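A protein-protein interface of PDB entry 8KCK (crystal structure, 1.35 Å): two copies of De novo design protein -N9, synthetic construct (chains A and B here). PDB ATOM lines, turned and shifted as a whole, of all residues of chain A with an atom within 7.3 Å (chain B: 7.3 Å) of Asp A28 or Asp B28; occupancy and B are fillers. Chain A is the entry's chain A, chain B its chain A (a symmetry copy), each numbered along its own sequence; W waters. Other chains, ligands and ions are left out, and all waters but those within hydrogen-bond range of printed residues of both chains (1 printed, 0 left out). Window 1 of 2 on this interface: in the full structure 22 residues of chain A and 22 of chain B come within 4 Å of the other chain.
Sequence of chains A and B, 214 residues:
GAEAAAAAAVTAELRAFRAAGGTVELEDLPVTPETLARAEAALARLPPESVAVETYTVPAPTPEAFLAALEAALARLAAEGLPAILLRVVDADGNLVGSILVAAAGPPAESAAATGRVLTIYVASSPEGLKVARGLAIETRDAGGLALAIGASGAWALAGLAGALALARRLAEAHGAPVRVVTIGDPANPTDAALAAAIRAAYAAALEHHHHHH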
ATOM      1  N   LEU A  26      11.816 -17.477  27.505  1.00  0.00           N
ATOM      2  CA  LEU A  26      12.831 -18.274  26.842  1.00  0.00           C
ATOM      3  C   LEU A  26      12.184 -19.554  26.315  1.00  0.00           C
ATOM      4  O   LEU A  26      11.536 -20.309  27.046  1.00  0.00           O
ATOM      5  CB  LEU A  26      14.017 -18.517  27.794  1.00  0.00           C
ATOM      6  CG  LEU A  26      15.224 -19.317  27.357  1.00  0.00           C
ATOM      7  CD1 LEU A  26      15.792 -18.867  25.967  1.00  0.00           C
ATOM      8  CD2 LEU A  26      16.321 -19.422  28.373  1.00  0.00           C
ATOM      9  N   GLU A  27      12.382 -19.816  25.036  1.00  0.00           N
ATOM     10  CA  GLU A  27      11.879 -20.982  24.332  1.00  0.00           C
ATOM     11  C   GLU A  27      13.041 -21.675  23.644  1.00  0.00           C
ATOM     12  O   GLU A  27      14.018 -21.024  23.231  1.00  0.00           O
ATOM     13  CB  GLU A  27      10.832 -20.495  23.326  1.00  0.00           C
ATOM     14  CG  GLU A  27      10.089 -21.516  22.587  1.00  0.00           C
ATOM     15  CD  GLU A  27       8.996 -20.933  21.694  1.00  0.00           C
ATOM     16  OE1 GLU A  27       8.972 -19.732  21.475  1.00  0.00           O
ATOM     17  OE2 GLU A  27       8.158 -21.712  21.205  1.00  0.00           O
ATOM     18  N   ASP A  28      12.967 -22.985  23.554  1.00  0.00           N
ATOM     19  CA  ASP A  28      13.927 -23.744  22.764  1.00  0.00           C
ATOM     20  C   ASP A  28      13.114 -24.614  21.844  1.00  0.00           C
ATOM     21  O   ASP A  28      12.223 -25.363  22.263  1.00  0.00           O
ATOM     22  CB  ASP A  28      14.850 -24.535  23.689  1.00  0.00           C
ATOM     23  CG  ASP A  28      15.486 -23.624  24.741  1.00  0.00           C
ATOM     24  OD1 ASP A  28      16.093 -22.590  24.387  1.00  0.00           O
ATOM     25  OD2 ASP A  28      15.366 -23.894  25.949  1.00  0.00           O
ATOM     26  N   LEU A  29      13.419 -24.485  20.557  1.00  0.00           N
ATOM     27  CA  LEU A  29      12.685 -25.220  19.539  1.00  0.00           C
ATOM     28  C   LEU A  29      13.631 -26.082  18.701  1.00  0.00           C
ATOM     29  O   LEU A  29      14.698 -25.633  18.296  1.00  0.00           O
ATOM     30  CB  LEU A  29      11.991 -24.270  18.574  1.00  0.00           C
ATOM     31  CG  LEU A  29      10.824 -23.461  19.152  1.00  0.00           C
ATOM     32  CD1 LEU A  29      10.117 -22.669  18.039  1.00  0.00           C
ATOM     33  CD2 LEU A  29       9.842 -24.334  19.975  1.00  0.00           C
ATOM     34  N   PRO A  30      13.253 -27.310  18.411  1.00  0.00           N
ATOM     35  CA  PRO A  30      14.053 -28.150  17.526  1.00  0.00           C
ATOM     36  C   PRO A  30      13.754 -27.862  16.076  1.00  0.00           C
ATOM     37  O   PRO A  30      12.635 -27.518  15.711  1.00  0.00           O
ATOM     38  CB  PRO A  30      13.570 -29.569  17.877  1.00  0.00           C
ATOM     39  CG  PRO A  30      12.065 -29.355  18.393  1.00  0.00           C
ATOM     40  CD  PRO A  30      12.121 -28.001  19.072  1.00  0.00           C
ATOM     41  N   VAL A 181      13.083 -14.961  23.681  1.00  0.00           N
ATOM     42  CA  VAL A 181      14.345 -15.498  23.188  1.00  0.00           C
ATOM     43  C   VAL A 181      14.071 -16.936  22.767  1.00  0.00           C
ATOM     44  O   VAL A 181      13.509 -17.708  23.542  1.00  0.00           O
ATOM     45  CB  VAL A 181      15.417 -15.512  24.284  1.00  0.00           C
ATOM     46  CG1 VAL A 181      16.703 -16.169  23.771  1.00  0.00           C
ATOM     47  CG2 VAL A 181      15.685 -14.094  24.829  1.00  0.00           C
ATOM     48  N   VAL A 182      14.456 -17.292  21.535  1.00  0.00           N
ATOM     49  CA  VAL A 182      14.149 -18.612  20.963  1.00  0.00           C
ATOM     50  C   VAL A 182      15.459 -19.225  20.472  1.00  0.00           C
ATOM     51  O   VAL A 182      16.029 -18.751  19.484  1.00  0.00           O
ATOM     52  CB  VAL A 182      13.127 -18.542  19.811  1.00  0.00           C
ATOM     53  CG1 VAL A 182      12.698 -19.950  19.355  1.00  0.00           C
ATOM     54  CG2 VAL A 182      11.926 -17.693  20.160  1.00  0.00           C
ATOM     55  N   THR A 183      15.943 -20.282  21.136  1.00  0.00           N
ATOM     56  CA  THR A 183      17.122 -20.985  20.615  1.00  0.00           C
ATOM     57  C   THR A 183      16.672 -22.150  19.746  1.00  0.00           C
ATOM     58  O   THR A 183      15.879 -22.991  20.175  1.00  0.00           O
ATOM     59  CB  THR A 183      18.004 -21.531  21.736  1.00  0.00           C
ATOM     60  OG1 THR A 183      17.345 -22.647  22.345  1.00  0.00           O
ATOM     61  CG2 THR A 183      18.315 -20.442  22.747  1.00  0.00           C
ATOM     62  N   ILE A 184      17.232 -22.217  18.547  1.00  0.00           N
ATOM     63  CA  ILE A 184      16.852 -23.209  17.545  1.00  0.00           C
ATOM     64  C   ILE A 184      18.016 -24.180  17.362  1.00  0.00           C
ATOM     65  O   ILE A 184      19.139 -23.727  17.116  1.00  0.00           O
ATOM     66  CB  ILE A 184      16.508 -22.552  16.206  1.00  0.00           C
ATOM     67  CG1 ILE A 184      15.490 -21.437  16.301  1.00  0.00           C
ATOM     68  CG2 ILE A 184      16.087 -23.624  15.202  1.00  0.00           C
ATOM     69  CD1 ILE A 184      14.158 -21.942  16.715  1.00  0.00           C
ATOM     70  N   GLY A 185      17.733 -25.470  17.473  1.00  0.00           N
ATOM     71  CA  GLY A 185      18.800 -26.444  17.320  1.00  0.00           C
ATOM     72  C   GLY A 185      18.399 -27.614  16.453  1.00  0.00           C
ATOM     73  O   GLY A 185      17.285 -28.162  16.565  1.00  0.00           O
ATOM     74  N   LEU A 195      25.021 -24.945  22.908  1.00  0.00           N
ATOM     75  CA  LEU A 195      24.580 -23.560  23.017  1.00  0.00           C
ATOM     76  C   LEU A 195      23.308 -23.468  23.855  1.00  0.00           C
ATOM     77  O   LEU A 195      23.189 -22.603  24.720  1.00  0.00           O
ATOM     78  CB  LEU A 195      24.325 -22.985  21.630  1.00  0.00           C
ATOM     79  CG  LEU A 195      23.797 -21.554  21.561  1.00  0.00           C
ATOM     80  CD1 LEU A 195      24.737 -20.615  22.275  1.00  0.00           C
ATOM     81  CD2 LEU A 195      23.662 -21.168  20.107  1.00  0.00           C
ATOM     82  N   ALA A 196      22.346 -24.342  23.593  1.00  0.00           N
ATOM     83  CA  ALA A 196      21.110 -24.287  24.348  1.00  0.00           C
ATOM     84  C   ALA A 196      21.385 -24.511  25.824  1.00  0.00           C
ATOM     85  O   ALA A 196      20.767 -23.853  26.678  1.00  0.00           O
ATOM     86  CB  ALA A 196      20.145 -25.328  23.795  1.00  0.00           C
ATOM     87  N   ALA A 197      22.290 -25.460  26.148  1.00  0.00           N
ATOM     88  CA  ALA A 197      22.596 -25.720  27.564  1.00  0.00           C
ATOM     89  C   ALA A 197      23.237 -24.502  28.200  1.00  0.00           C
ATOM     90  O   ALA A 197      22.927 -24.156  29.340  1.00  0.00           O
ATOM     91  CB  ALA A 197      23.529 -26.904  27.692  1.00  0.00           C
ATOM     92  N   ILE A 199      22.828 -21.334  27.316  1.00  0.00           N
ATOM     93  CA  ILE A 199      21.835 -20.281  27.521  1.00  0.00           C
ATOM     94  C   ILE A 199      20.911 -20.600  28.679  1.00  0.00           C
ATOM     95  O   ILE A 199      20.578 -19.713  29.468  1.00  0.00           O
ATOM     96  CB  ILE A 199      21.072 -20.046  26.203  1.00  0.00           C
ATOM     97  CG1 ILE A 199      22.022 -19.365  25.209  1.00  0.00           C
ATOM     98  CG2 ILE A 199      19.912 -19.146  26.393  1.00  0.00           C
ATOM     99  CD1 ILE A 199      21.464 -19.293  23.747  1.00  0.00           C
ATOM    100  N   ARG A 200      20.484 -21.855  28.799  1.00  0.00           N
ATOM    101  CA  ARG A 200      19.639 -22.221  29.936  1.00  0.00           C
ATOM    102  C   ARG A 200      20.355 -22.063  31.260  1.00  0.00           C
ATOM    103  O   ARG A 200      19.749 -21.659  32.250  1.00  0.00           O
ATOM    104  CB  ARG A 200      19.138 -23.662  29.825  1.00  0.00           C
ATOM    105  CG  ARG A 200      18.258 -23.957  28.659  1.00  0.00           C
ATOM    106  CD  ARG A 200      17.141 -23.013  28.447  1.00  0.00           C
ATOM    107  NE  ARG A 200      16.238 -22.871  29.582  1.00  0.00           N
ATOM    108  CZ  ARG A 200      14.941 -22.590  29.464  1.00  0.00           C
ATOM    109  NH1 ARG A 200      14.339 -22.574  28.282  1.00  0.00           N
ATOM    110  NH2 ARG A 200      14.250 -22.271  30.548  1.00  0.00           N
ATOM    111  N   LEU B  26      13.650 -32.152  21.582  1.00  0.00           N
ATOM    112  CA  LEU B  26      13.567 -31.491  22.870  1.00  0.00           C
ATOM    113  C   LEU B  26      13.108 -30.049  22.655  1.00  0.00           C
ATOM    114  O   LEU B  26      13.693 -29.286  21.882  1.00  0.00           O
ATOM    115  CB  LEU B  26      14.909 -31.618  23.615  1.00  0.00           C
ATOM    116  CG  LEU B  26      15.102 -31.022  24.992  1.00  0.00           C
ATOM    117  CD1 LEU B  26      13.949 -31.386  25.989  1.00  0.00           C
ATOM    118  CD2 LEU B  26      16.443 -31.273  25.613  1.00  0.00           C
ATOM    119  N   GLU B  27      12.065 -29.664  23.366  1.00  0.00           N
ATOM    120  CA  GLU B  27      11.474 -28.339  23.336  1.00  0.00           C
ATOM    121  C   GLU B  27      11.400 -27.805  24.754  1.00  0.00           C
ATOM    122  O   GLU B  27      11.245 -28.575  25.719  1.00  0.00           O
ATOM    123  CB  GLU B  27      10.085 -28.469  22.705  1.00  0.00           C
ATOM    124  CG  GLU B  27       9.346 -27.232  22.450  1.00  0.00           C
ATOM    125  CD  GLU B  27       8.024 -27.462  21.722  1.00  0.00           C
ATOM    126  OE1 GLU B  27       7.577 -28.594  21.624  1.00  0.00           O
ATOM    127  OE2 GLU B  27       7.432 -26.475  21.249  1.00  0.00           O
ATOM    128  N   ASP B  28      11.552 -26.506  24.896  1.00  0.00           N
ATOM    129  CA  ASP B  28      11.325 -25.854  26.179  1.00  0.00           C
ATOM    130  C   ASP B  28      10.368 -24.725  25.910  1.00  0.00           C
ATOM    131  O   ASP B  28      10.580 -23.877  25.035  1.00  0.00           O
ATOM    132  CB  ASP B  28      12.657 -25.392  26.768  1.00  0.00           C
ATOM    133  CG  ASP B  28      13.665 -26.544  26.819  1.00  0.00           C
ATOM    134  OD1 ASP B  28      13.354 -27.620  27.372  1.00  0.00           O
ATOM    135  OD2 ASP B  28      14.777 -26.418  26.277  1.00  0.00           O
ATOM    136  N   LEU B  29       9.278 -24.740  26.670  1.00  0.00           N
ATOM    137  CA  LEU B  29       8.232 -23.745  26.493  1.00  0.00           C
ATOM    138  C   LEU B  29       7.977 -22.983  27.795  1.00  0.00           C
ATOM    139  O   LEU B  29       7.902 -23.578  28.866  1.00  0.00           O
ATOM    140  CB  LEU B  29       6.914 -24.401  26.107  1.00  0.00           C
ATOM    141  CG  LEU B  29       6.863 -25.032  24.710  1.00  0.00           C
ATOM    142  CD1 LEU B  29       5.436 -25.512  24.391  1.00  0.00           C
ATOM    143  CD2 LEU B  29       7.434 -24.099  23.612  1.00  0.00           C
ATOM    144  N   PRO B  30       7.821 -21.677  27.726  1.00  0.00           N
ATOM    145  CA  PRO B  30       7.467 -20.903  28.911  1.00  0.00           C
ATOM    146  C   PRO B  30       5.980 -20.930  29.161  1.00  0.00           C
ATOM    147  O   PRO B  30       5.178 -20.993  28.236  1.00  0.00           O
ATOM    148  CB  PRO B  30       7.896 -19.476  28.523  1.00  0.00           C
ATOM    149  CG  PRO B  30       7.784 -19.453  26.922  1.00  0.00           C
ATOM    150  CD  PRO B  30       8.155 -20.870  26.529  1.00  0.00           C
ATOM    151  N   VAL B 181      10.117 -34.337  23.884  1.00  0.00           N
ATOM    152  CA  VAL B 181      10.227 -34.000  25.297  1.00  0.00           C
ATOM    153  C   VAL B 181      10.029 -32.493  25.402  1.00  0.00           C
ATOM    154  O   VAL B 181      10.688 -31.736  24.693  1.00  0.00           O
ATOM    155  CB  VAL B 181      11.613 -34.346  25.853  1.00  0.00           C
ATOM    156  CG1 VAL B 181      11.737 -33.895  27.312  1.00  0.00           C
ATOM    157  CG2 VAL B 181      11.926 -35.848  25.697  1.00  0.00           C
ATOM    158  N   VAL B 182       9.114 -32.060  26.279  1.00  0.00           N
ATOM    159  CA  VAL B 182       8.744 -30.642  26.396  1.00  0.00           C
ATOM    160  C   VAL B 182       8.888 -30.241  27.863  1.00  0.00           C
ATOM    161  O   VAL B 182       8.097 -30.682  28.703  1.00  0.00           O
ATOM    162  CB  VAL B 182       7.313 -30.353  25.901  1.00  0.00           C
ATOM    163  CG1 VAL B 182       7.023 -28.840  25.873  1.00  0.00           C
ATOM    164  CG2 VAL B 182       7.033 -30.986  24.557  1.00  0.00           C
ATOM    165  N   THR B 183       9.876 -29.399  28.188  1.00  0.00           N
ATOM    166  CA  THR B 183       9.963 -28.881  29.559  1.00  0.00           C
ATOM    167  C   THR B 183       9.241 -27.544  29.640  1.00  0.00           C
ATOM    168  O   THR B 183       9.515 -26.627  28.862  1.00  0.00           O
ATOM    169  CB  THR B 183      11.411 -28.675  30.001  1.00  0.00           C
ATOM    170  OG1 THR B 183      11.951 -27.542  29.313  1.00  0.00           O
ATOM    171  CG2 THR B 183      12.229 -29.929  29.748  1.00  0.00           C
ATOM    172  N   ILE B 184       8.361 -27.431  30.625  1.00  0.00           N
ATOM    173  CA  ILE B 184       7.508 -26.258  30.798  1.00  0.00           C
ATOM    174  C   ILE B 184       7.950 -25.523  32.060  1.00  0.00           C
ATOM    175  O   ILE B 184       8.039 -26.152  33.120  1.00  0.00           O
ATOM    176  CB  ILE B 184       6.033 -26.650  30.916  1.00  0.00           C
ATOM    177  CG1 ILE B 184       5.533 -27.544  29.802  1.00  0.00           C
ATOM    178  CG2 ILE B 184       5.178 -25.392  31.063  1.00  0.00           C
ATOM    179  CD1 ILE B 184       5.533 -26.843  28.493  1.00  0.00           C
ATOM    180  N   GLY B 185       8.206 -24.228  31.931  1.00  0.00           N
ATOM    181  CA  GLY B 185       8.643 -23.474  33.094  1.00  0.00           C
ATOM    182  C   GLY B 185       7.940 -22.142  33.219  1.00  0.00           C
ATOM    183  O   GLY B 185       7.751 -21.404  32.233  1.00  0.00           O
ATOM    184  N   LEU B 195      15.673 -26.908  36.404  1.00  0.00           N
ATOM    185  CA  LEU B 195      15.339 -28.180  35.774  1.00  0.00           C
ATOM    186  C   LEU B 195      15.629 -28.128  34.277  1.00  0.00           C
ATOM    187  O   LEU B 195      16.204 -29.060  33.718  1.00  0.00           O
ATOM    188  CB  LEU B 195      13.869 -28.502  36.002  1.00  0.00           C
ATOM    189  CG  LEU B 195      13.332 -29.779  35.357  1.00  0.00           C
ATOM    190  CD1 LEU B 195      14.135 -30.972  35.813  1.00  0.00           C
ATOM    191  CD2 LEU B 195      11.881 -29.933  35.745  1.00  0.00           C
ATOM    192  N   ALA B 196      15.219 -27.054  33.618  1.00  0.00           N
ATOM    193  CA  ALA B 196      15.453 -26.963  32.190  1.00  0.00           C
ATOM    194  C   ALA B 196      16.943 -26.996  31.899  1.00  0.00           C
ATOM    195  O   ALA B 196      17.370 -27.627  30.916  1.00  0.00           O
ATOM    196  CB  ALA B 196      14.810 -25.687  31.662  1.00  0.00           C
ATOM    197  N   ALA B 197      17.751 -26.298  32.725  1.00  0.00           N
ATOM    198  CA  ALA B 197      19.204 -26.295  32.490  1.00  0.00           C
ATOM    199  C   ALA B 197      19.773 -27.689  32.666  1.00  0.00           C
ATOM    200  O   ALA B 197      20.633 -28.115  31.896  1.00  0.00           O
ATOM    201  CB  ALA B 197      19.891 -25.347  33.449  1.00  0.00           C
ATOM    202  N   ILE B 199      18.191 -30.567  32.213  1.00  0.00           N
ATOM    203  CA  ILE B 199      17.814 -31.419  31.088  1.00  0.00           C
ATOM    204  C   ILE B 199      18.601 -31.081  29.839  1.00  0.00           C
ATOM    205  O   ILE B 199      19.026 -31.981  29.112  1.00  0.00           O
ATOM    206  CB  ILE B 199      16.291 -31.321  30.871  1.00  0.00           C
ATOM    207  CG1 ILE B 199      15.590 -32.038  32.032  1.00  0.00           C
ATOM    208  CG2 ILE B 199      15.869 -31.990  29.620  1.00  0.00           C
ATOM    209  CD1 ILE B 199      14.041 -31.803  32.080  1.00  0.00           C
ATOM    210  N   ARG B 200      18.807 -29.794  29.570  1.00  0.00           N
ATOM    211  CA  ARG B 200      19.614 -29.421  28.408  1.00  0.00           C
ATOM    212  C   ARG B 200      21.046 -29.893  28.526  1.00  0.00           C
ATOM    213  O   ARG B 200      21.652 -30.297  27.536  1.00  0.00           O
ATOM    214  CB  ARG B 200      19.619 -27.908  28.186  1.00  0.00           C
ATOM    215  CG  ARG B 200      18.298 -27.291  27.874  1.00  0.00           C
ATOM    216  CD  ARG B 200      17.517 -27.959  26.811  1.00  0.00           C
ATOM    217  NE  ARG B 200      18.200 -28.068  25.529  1.00  0.00           N
ATOM    218  CZ  ARG B 200      17.572 -28.068  24.354  1.00  0.00           C
ATOM    219  NH1 ARG B 200      16.275 -27.807  24.261  1.00  0.00           N
ATOM    220  NH2 ARG B 200      18.250 -28.385  23.261  1.00  0.00           N
HETATM  221  O   HOH W   1      22.716 -26.272  31.246  1.00  0.00           O
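Water W1 lies within hydrogen-bond range of the backbone carbonyl oxygen (O) of Ala A197 and the backbone carbonyl oxygen (O) of Ala B197.
Printed residues of chain B that touch a printed residue of chain A: Leu B26, Glu B27, Asp B28, Leu B29, Pro B30, Ala B196, Ala B197 and Arg B200.
Hydrophobic or aromatic side chains of chain B within 4 Å of the printed part of chain A: Leu B29, Pro B30, Ala B196 and Ala B197.
Along chain B the printed residues that touch a printed residue of chain A span positions 26 to 200.
Among the printed residues, no Asp or Glu carboxylate lies within 4 Å of a Lys or Arg side-chain nitrogen of the other chain.
Leu A26 touches Pro B30, and with the chains exchanged Pro A30 touches Leu B26.
Glu A27 touches Asp B28, and with the chains exchanged Asp A28 touches Glu B27.
Asp B28 touches its own counterpart, Asp A28.
Asp A28 touches Arg B200, and with the chains exchanged Arg A200 touches Asp B28.
Positions printed for both chains: 26, 27, 28, 29, 30, 181, 182, 183, 184, 185, 195, 196, 197, 199 and 200.
Asp A28 touches just these residues of chain B: Glu B27, Asp B28 and Arg B200.
Of the printed residues of chain B, Pro A30 touches Leu B26 (3.5 Å).
Of the printed residues of chain B, Arg A200 touches Asp B28 (3.6 Å), Ala B196 (3.6 Å), Ala B197 (3.7 Å) and Arg B200 (3.4 Å).
Of chain A, only Glu A27, Asp A28 and Arg A200 come within 4 Å of Asp B28.
Of the printed residues of chain A, Arg B200 touches Asp A28, Ala A196, Ala A197 and Arg A200.
The nearest residue of chain B that does not touch Asp A28 is Leu B26 (4.2 Å).
The nearest printed residue of chain A that does not touch Arg B200 is Thr A183 (5.6 Å).
The backbone NH of Glu A27 is in hydrogen-bond range of the backbone carbonyl oxygen of Val A181 (2.8 Å).
O of Glu A27 lies within hydrogen-bond range of N of Thr A183.
N of Gly A185 is in hydrogen-bond range of O of Leu A29, 3.1 Å away.
The backbone NH (N) of Glu B27 is in hydrogen-bond range of the backbone carbonyl oxygen (O) of Val B181 (2.8 Å).
The backbone NH of Thr B183 lies within hydrogen-bond range of the backbone carbonyl oxygen of Glu B27.
NH1 of Arg B200 lies within salt-bridge range of OD2 of Asp B28 (2.9 Å).
The backbone carbonyl oxygen of Asp A28 is in hydrogen-bond range of the backbone NH of Asp B28 (2.9 Å).
Among the printed residues, pairs that only touch across the chains: Glu A27 with Asp B28, Asp A28 with Glu B27, Arg A200 with Arg B200, Leu A26 with Pro B30, Leu A29 with Glu B27, Glu A27 with Leu B29, Pro A30 with Leu B26, Arg A200 with Asp B28, Asp A28 with Arg B200, Ala A196 with Arg B200, Arg A200 with Ala B196, Ala A197 with Arg B200 and Arg A200 with Ala B197.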
